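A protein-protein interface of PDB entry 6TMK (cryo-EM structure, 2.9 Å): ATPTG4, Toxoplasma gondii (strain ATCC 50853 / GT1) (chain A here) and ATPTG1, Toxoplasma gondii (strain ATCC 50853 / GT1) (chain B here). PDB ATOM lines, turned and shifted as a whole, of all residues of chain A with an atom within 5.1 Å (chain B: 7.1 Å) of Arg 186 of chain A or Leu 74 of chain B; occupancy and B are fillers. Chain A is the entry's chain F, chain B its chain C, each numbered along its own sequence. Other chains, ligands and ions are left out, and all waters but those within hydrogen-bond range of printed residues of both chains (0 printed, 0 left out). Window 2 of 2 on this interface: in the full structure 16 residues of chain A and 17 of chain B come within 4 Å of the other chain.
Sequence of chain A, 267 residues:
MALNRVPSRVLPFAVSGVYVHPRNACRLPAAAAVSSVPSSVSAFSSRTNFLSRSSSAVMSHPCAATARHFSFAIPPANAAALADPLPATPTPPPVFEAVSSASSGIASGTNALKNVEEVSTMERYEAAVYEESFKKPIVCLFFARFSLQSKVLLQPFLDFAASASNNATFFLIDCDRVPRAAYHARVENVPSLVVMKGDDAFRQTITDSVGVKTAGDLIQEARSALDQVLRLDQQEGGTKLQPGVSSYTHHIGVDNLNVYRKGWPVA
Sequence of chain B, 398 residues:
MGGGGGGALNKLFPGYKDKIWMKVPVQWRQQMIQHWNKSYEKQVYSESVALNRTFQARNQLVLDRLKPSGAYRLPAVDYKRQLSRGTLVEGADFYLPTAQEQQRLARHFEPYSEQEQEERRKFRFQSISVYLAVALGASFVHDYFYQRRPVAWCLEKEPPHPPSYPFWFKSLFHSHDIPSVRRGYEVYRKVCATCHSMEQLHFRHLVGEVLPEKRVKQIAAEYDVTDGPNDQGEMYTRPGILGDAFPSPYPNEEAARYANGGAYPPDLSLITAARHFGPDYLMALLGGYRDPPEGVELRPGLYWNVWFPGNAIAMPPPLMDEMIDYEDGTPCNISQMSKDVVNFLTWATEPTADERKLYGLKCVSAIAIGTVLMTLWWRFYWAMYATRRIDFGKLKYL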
ATOM      1  N   ALA A 182      18.965 -15.187 -24.008  1.00  0.00           N
ATOM      2  CA  ALA A 182      19.220 -15.563 -22.626  1.00  0.00           C
ATOM      3  C   ALA A 182      18.023 -16.281 -22.027  1.00  0.00           C
ATOM      4  O   ALA A 182      18.181 -17.239 -21.264  1.00  0.00           O
ATOM      5  CB  ALA A 182      19.568 -14.326 -21.814  1.00  0.00           C
ATOM      6  N   TYR A 183      16.816 -15.831 -22.366  1.00  0.00           N
ATOM      7  CA  TYR A 183      15.616 -16.529 -21.931  1.00  0.00           C
ATOM      8  C   TYR A 183      15.540 -17.916 -22.547  1.00  0.00           C
ATOM      9  O   TYR A 183      15.064 -18.863 -21.914  1.00  0.00           O
ATOM     10  CB  TYR A 183      14.384 -15.719 -22.314  1.00  0.00           C
ATOM     11  CG  TYR A 183      14.384 -14.307 -21.797  1.00  0.00           C
ATOM     12  CD1 TYR A 183      15.066 -13.969 -20.647  1.00  0.00           C
ATOM     13  CD2 TYR A 183      13.690 -13.311 -22.456  1.00  0.00           C
ATOM     14  CE1 TYR A 183      15.061 -12.685 -20.173  1.00  0.00           C
ATOM     15  CE2 TYR A 183      13.683 -12.026 -21.989  1.00  0.00           C
ATOM     16  CZ  TYR A 183      14.368 -11.718 -20.845  1.00  0.00           C
ATOM     17  OH  TYR A 183      14.362 -10.433 -20.371  1.00  0.00           O
ATOM     18  N   HIS A 184      16.009 -18.049 -23.784  1.00  0.00           N
ATOM     19  CA  HIS A 184      15.996 -19.339 -24.459  1.00  0.00           C
ATOM     20  C   HIS A 184      16.893 -20.341 -23.751  1.00  0.00           C
ATOM     21  O   HIS A 184      16.487 -21.477 -23.484  1.00  0.00           O
ATOM     22  CB  HIS A 184      16.441 -19.147 -25.905  1.00  0.00           C
ATOM     23  CG  HIS A 184      16.452 -20.404 -26.710  1.00  0.00           C
ATOM     24  ND1 HIS A 184      17.410 -21.380 -26.549  1.00  0.00           N
ATOM     25  CD2 HIS A 184      15.642 -20.833 -27.703  1.00  0.00           C
ATOM     26  CE1 HIS A 184      17.178 -22.365 -27.397  1.00  0.00           C
ATOM     27  NE2 HIS A 184      16.110 -22.057 -28.109  1.00  0.00           N
ATOM     28  N   ALA A 185      18.121 -19.939 -23.443  1.00  0.00           N
ATOM     29  CA  ALA A 185      19.087 -20.821 -22.813  1.00  0.00           C
ATOM     30  C   ALA A 185      18.850 -21.013 -21.322  1.00  0.00           C
ATOM     31  O   ALA A 185      19.565 -21.805 -20.701  1.00  0.00           O
ATOM     32  CB  ALA A 185      20.489 -20.277 -23.042  1.00  0.00           C
ATOM     33  N   ARG A 186      17.881 -20.315 -20.735  1.00  0.00           N
ATOM     34  CA  ARG A 186      17.535 -20.500 -19.329  1.00  0.00           C
ATOM     35  C   ARG A 186      18.703 -20.121 -18.429  1.00  0.00           C
ATOM     36  O   ARG A 186      19.009 -20.807 -17.452  1.00  0.00           O
ATOM     37  CB  ARG A 186      17.077 -21.931 -19.047  1.00  0.00           C
ATOM     38  CG  ARG A 186      16.016 -22.449 -19.983  1.00  0.00           C
ATOM     39  CD  ARG A 186      14.751 -21.642 -19.902  1.00  0.00           C
ATOM     40  NE  ARG A 186      14.139 -21.668 -18.579  1.00  0.00           N
ATOM     41  CZ  ARG A 186      13.412 -22.673 -18.106  1.00  0.00           C
ATOM     42  NH1 ARG A 186      12.897 -22.594 -16.892  1.00  0.00           N
ATOM     43  NH2 ARG A 186      13.207 -23.755 -18.837  1.00  0.00           N
ATOM     44  N   VAL A 187      19.356 -19.015 -18.753  1.00  0.00           N
ATOM     45  CA  VAL A 187      20.438 -18.486 -17.936  1.00  0.00           C
ATOM     46  C   VAL A 187      19.849 -17.554 -16.890  1.00  0.00           C
ATOM     47  O   VAL A 187      19.032 -16.681 -17.208  1.00  0.00           O
ATOM     48  CB  VAL A 187      21.478 -17.755 -18.801  1.00  0.00           C
ATOM     49  CG1 VAL A 187      21.908 -18.615 -19.957  1.00  0.00           C
ATOM     50  CG2 VAL A 187      20.940 -16.454 -19.291  1.00  0.00           C
ATOM     51  N   GLU A 188      20.257 -17.750 -15.637  1.00  0.00           N
ATOM     52  CA  GLU A 188      19.802 -16.923 -14.534  1.00  0.00           C
ATOM     53  C   GLU A 188      20.905 -16.074 -13.930  1.00  0.00           C
ATOM     54  O   GLU A 188      20.602 -15.079 -13.265  1.00  0.00           O
ATOM     55  CB  GLU A 188      19.201 -17.798 -13.426  1.00  0.00           C
ATOM     56  CG  GLU A 188      17.916 -18.515 -13.802  1.00  0.00           C
ATOM     57  CD  GLU A 188      18.157 -19.823 -14.526  1.00  0.00           C
ATOM     58  OE1 GLU A 188      19.334 -20.200 -14.705  1.00  0.00           O
ATOM     59  OE2 GLU A 188      17.169 -20.479 -14.913  1.00  0.00           O
ATOM     60  N   ARG A 203      21.924 -30.004 -23.775  1.00  0.00           N
ATOM     61  CA  ARG A 203      22.088 -28.640 -23.289  1.00  0.00           C
ATOM     62  C   ARG A 203      22.693 -28.721 -21.899  1.00  0.00           C
ATOM     63  O   ARG A 203      22.054 -29.221 -20.969  1.00  0.00           O
ATOM     64  CB  ARG A 203      20.765 -27.886 -23.270  1.00  0.00           C
ATOM     65  CG  ARG A 203      20.932 -26.400 -23.101  1.00  0.00           C
ATOM     66  CD  ARG A 203      19.601 -25.708 -23.035  1.00  0.00           C
ATOM     67  NE  ARG A 203      18.932 -25.716 -24.328  1.00  0.00           N
ATOM     68  CZ  ARG A 203      17.868 -24.980 -24.620  1.00  0.00           C
ATOM     69  NH1 ARG A 203      17.350 -24.172 -23.711  1.00  0.00           N
ATOM     70  NH2 ARG A 203      17.324 -25.052 -25.822  1.00  0.00           N
ATOM     71  N   VAL A 254       8.548 -20.915 -22.172  1.00  0.00           N
ATOM     72  CA  VAL A 254       9.707 -20.133 -21.774  1.00  0.00           C
ATOM     73  C   VAL A 254       9.586 -18.708 -22.290  1.00  0.00           C
ATOM     74  O   VAL A 254       9.810 -17.741 -21.555  1.00  0.00           O
ATOM     75  CB  VAL A 254      10.985 -20.811 -22.290  1.00  0.00           C
ATOM     76  CG1 VAL A 254      12.184 -19.928 -22.076  1.00  0.00           C
ATOM     77  CG2 VAL A 254      11.170 -22.147 -21.627  1.00  0.00           C
ATOM     78  N   GLY B  70      19.172 -30.533 -13.978  1.00  0.00           N
ATOM     79  CA  GLY B  70      18.600 -29.435 -14.734  1.00  0.00           C
ATOM     80  C   GLY B  70      18.215 -29.799 -16.151  1.00  0.00           C
ATOM     81  O   GLY B  70      17.608 -28.971 -16.846  1.00  0.00           O
ATOM     82  N   ALA B  71      18.548 -31.005 -16.611  1.00  0.00           N
ATOM     83  CA  ALA B  71      18.125 -31.445 -17.934  1.00  0.00           C
ATOM     84  C   ALA B  71      16.615 -31.605 -18.011  1.00  0.00           C
ATOM     85  O   ALA B  71      15.990 -31.214 -19.003  1.00  0.00           O
ATOM     86  CB  ALA B  71      18.809 -32.761 -18.282  1.00  0.00           C
ATOM     87  N   TYR B  72      16.016 -32.179 -16.972  1.00  0.00           N
ATOM     88  CA  TYR B  72      14.590 -32.463 -16.923  1.00  0.00           C
ATOM     89  C   TYR B  72      13.823 -31.396 -16.157  1.00  0.00           C
ATOM     90  O   TYR B  72      12.800 -31.687 -15.530  1.00  0.00           O
ATOM     91  CB  TYR B  72      14.356 -33.839 -16.310  1.00  0.00           C
ATOM     92  CG  TYR B  72      15.172 -34.934 -16.954  1.00  0.00           C
ATOM     93  CD1 TYR B  72      14.921 -35.333 -18.256  1.00  0.00           C
ATOM     94  CD2 TYR B  72      16.194 -35.562 -16.267  1.00  0.00           C
ATOM     95  CE1 TYR B  72      15.659 -36.326 -18.849  1.00  0.00           C
ATOM     96  CE2 TYR B  72      16.938 -36.557 -16.852  1.00  0.00           C
ATOM     97  CZ  TYR B  72      16.666 -36.937 -18.144  1.00  0.00           C
ATOM     98  OH  TYR B  72      17.410 -37.931 -18.735  1.00  0.00           O
ATOM     99  N   ARG B  73      14.305 -30.161 -16.198  1.00  0.00           N
ATOM    100  CA  ARG B  73      13.640 -29.071 -15.513  1.00  0.00           C
ATOM    101  C   ARG B  73      12.290 -28.767 -16.150  1.00  0.00           C
ATOM    102  O   ARG B  73      11.920 -29.298 -17.200  1.00  0.00           O
ATOM    103  CB  ARG B  73      14.508 -27.818 -15.538  1.00  0.00           C
ATOM    104  CG  ARG B  73      14.701 -27.236 -16.919  1.00  0.00           C
ATOM    105  CD  ARG B  73      15.829 -26.240 -16.938  1.00  0.00           C
ATOM    106  NE  ARG B  73      15.578 -25.123 -16.040  1.00  0.00           N
ATOM    107  CZ  ARG B  73      16.417 -24.110 -15.866  1.00  0.00           C
ATOM    108  NH1 ARG B  73      17.563 -24.079 -16.529  1.00  0.00           N
ATOM    109  NH2 ARG B  73      16.108 -23.130 -15.030  1.00  0.00           N
ATOM    110  N   LEU B  74      11.555 -27.895 -15.489  1.00  0.00           N
ATOM    111  CA  LEU B  74      10.252 -27.484 -15.976  1.00  0.00           C
ATOM    112  C   LEU B  74      10.429 -26.660 -17.244  1.00  0.00           C
ATOM    113  O   LEU B  74      11.168 -25.670 -17.233  1.00  0.00           O
ATOM    114  CB  LEU B  74       9.519 -26.689 -14.909  1.00  0.00           C
ATOM    115  CG  LEU B  74       8.009 -26.548 -15.084  1.00  0.00           C
ATOM    116  CD1 LEU B  74       7.313 -26.508 -13.761  1.00  0.00           C
ATOM    117  CD2 LEU B  74       7.683 -25.300 -15.818  1.00  0.00           C
ATOM    118  N   PRO B  75       9.766 -27.013 -18.342  1.00  0.00           N
ATOM    119  CA  PRO B  75       9.972 -26.321 -19.617  1.00  0.00           C
ATOM    120  C   PRO B  75       9.092 -25.091 -19.794  1.00  0.00           C
ATOM    121  O   PRO B  75       8.399 -24.934 -20.803  1.00  0.00           O
ATOM    122  CB  PRO B  75       9.639 -27.409 -20.639  1.00  0.00           C
ATOM    123  CG  PRO B  75       8.539 -28.161 -19.989  1.00  0.00           C
ATOM    124  CD  PRO B  75       8.746 -28.067 -18.489  1.00  0.00           C
ATOM    125  N   ALA B  76       9.114 -24.204 -18.805  1.00  0.00           N
ATOM    126  CA  ALA B  76       8.283 -23.011 -18.840  1.00  0.00           C
ATOM    127  C   ALA B  76       8.777 -22.042 -17.777  1.00  0.00           C
ATOM    128  O   ALA B  76       9.573 -22.393 -16.904  1.00  0.00           O
ATOM    129  CB  ALA B  76       6.814 -23.359 -18.621  1.00  0.00           C
ATOM    130  N   VAL B  77       8.278 -20.813 -17.865  1.00  0.00           N
ATOM    131  CA  VAL B  77       8.619 -19.736 -16.950  1.00  0.00           C
ATOM    132  C   VAL B  77       7.324 -19.130 -16.434  1.00  0.00           C
ATOM    133  O   VAL B  77       6.339 -19.031 -17.171  1.00  0.00           O
ATOM    134  CB  VAL B  77       9.494 -18.667 -17.635  1.00  0.00           C
ATOM    135  CG1 VAL B  77       9.753 -17.508 -16.707  1.00  0.00           C
ATOM    136  CG2 VAL B  77      10.795 -19.263 -18.097  1.00  0.00           C
ATOM    137  N   ASP B  78       7.325 -18.728 -15.168  1.00  0.00           N
ATOM    138  CA  ASP B  78       6.098 -18.260 -14.546  1.00  0.00           C
ATOM    139  C   ASP B  78       5.591 -16.984 -15.210  1.00  0.00           C
ATOM    140  O   ASP B  78       6.355 -16.184 -15.763  1.00  0.00           O
ATOM    141  CB  ASP B  78       6.316 -18.036 -13.052  1.00  0.00           C
ATOM    142  CG  ASP B  78       7.472 -17.113 -12.761  1.00  0.00           C
ATOM    143  OD1 ASP B  78       7.233 -15.908 -12.537  1.00  0.00           O
ATOM    144  OD2 ASP B  78       8.622 -17.595 -12.755  1.00  0.00           O
ATOM    145  N   ARG B  85       9.326  -9.502 -17.978  1.00  0.00           N
ATOM    146  CA  ARG B  85      10.203  -9.519 -19.140  1.00  0.00           C
ATOM    147  C   ARG B  85       9.573  -8.864 -20.357  1.00  0.00           C
ATOM    148  O   ARG B  85      10.289  -8.550 -21.312  1.00  0.00           O
ATOM    149  CB  ARG B  85      10.581 -10.952 -19.492  1.00  0.00           C
ATOM    150  CG  ARG B  85      11.559 -11.588 -18.561  1.00  0.00           C
ATOM    151  CD  ARG B  85      11.569 -13.071 -18.736  1.00  0.00           C
ATOM    152  NE  ARG B  85      12.665 -13.700 -18.018  1.00  0.00           N
ATOM    153  CZ  ARG B  85      13.059 -14.949 -18.217  1.00  0.00           C
ATOM    154  NH1 ARG B  85      14.064 -15.440 -17.522  1.00  0.00           N
ATOM    155  NH2 ARG B  85      12.459 -15.699 -19.124  1.00  0.00           N
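Of the 9 printed residues of chain A, 4 touch a printed residue of chain B. Among the printed residues, Asp or Glu carboxylates within 4 Å of a Lys or Arg side-chain nitrogen of the other chain: Glu 188 of chain A with Arg 73 of chain B (2.9 Å).
Tyr 183 of chain A touches Arg 85 of chain B. Arg 73 of chain B touches Arg 186 of chain A (NH1 to CB, 3.3 Å). Val 254 of chain A touches Ala 76 of chain B (N to CA, 3.9 Å). Val 254 of chain A touches Val 77 of chain B (O to CG2, 3.9 Å).
Printed residues of chain B within 4 Å of Tyr 183 of chain A: Arg 85 (3.3 Å). Of the printed residues of chain B, Arg 186 of chain A touches Arg 73 (3.3 Å), Leu 74 (3.2 Å) and Ala 76 (3.3 Å). Of the printed residues of chain B, Glu 188 of chain A touches Arg 73 (2.9 Å). Arg 203 of chain A touches none of the printed residues of chain B. Of chain A, only Arg 186 comes within 4 Å of Leu 74 of chain B. Pro 75 of chain B touches none of the printed residues of chain A. Of the printed residues of chain A, Ala 76 of chain B touches Arg 186 (3.3 Å) and Val 254 (3.9 Å). The nearest printed residue of chain A that does not touch Leu 74 of chain B is Val 254 of chain A (5.6 Å). The nearest printed residue of chain B that does not touch Glu 188 of chain A is Arg 85 of chain B (6.2 Å).
OE2 of Glu 188 of chain A is in salt-bridge range of NH2 of Arg 73 of chain B (2.9 Å). O of Leu 74 of chain B lies within hydrogen-bond range of NH2 of Arg 186 of chain A, 3.2 Å away. The guanidinium group (NH1) of Arg 186 of chain A sits at hydrogen-bond distance from the backbone carbonyl oxygen (O) of Ala 76 of chain B (3.3 Å).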
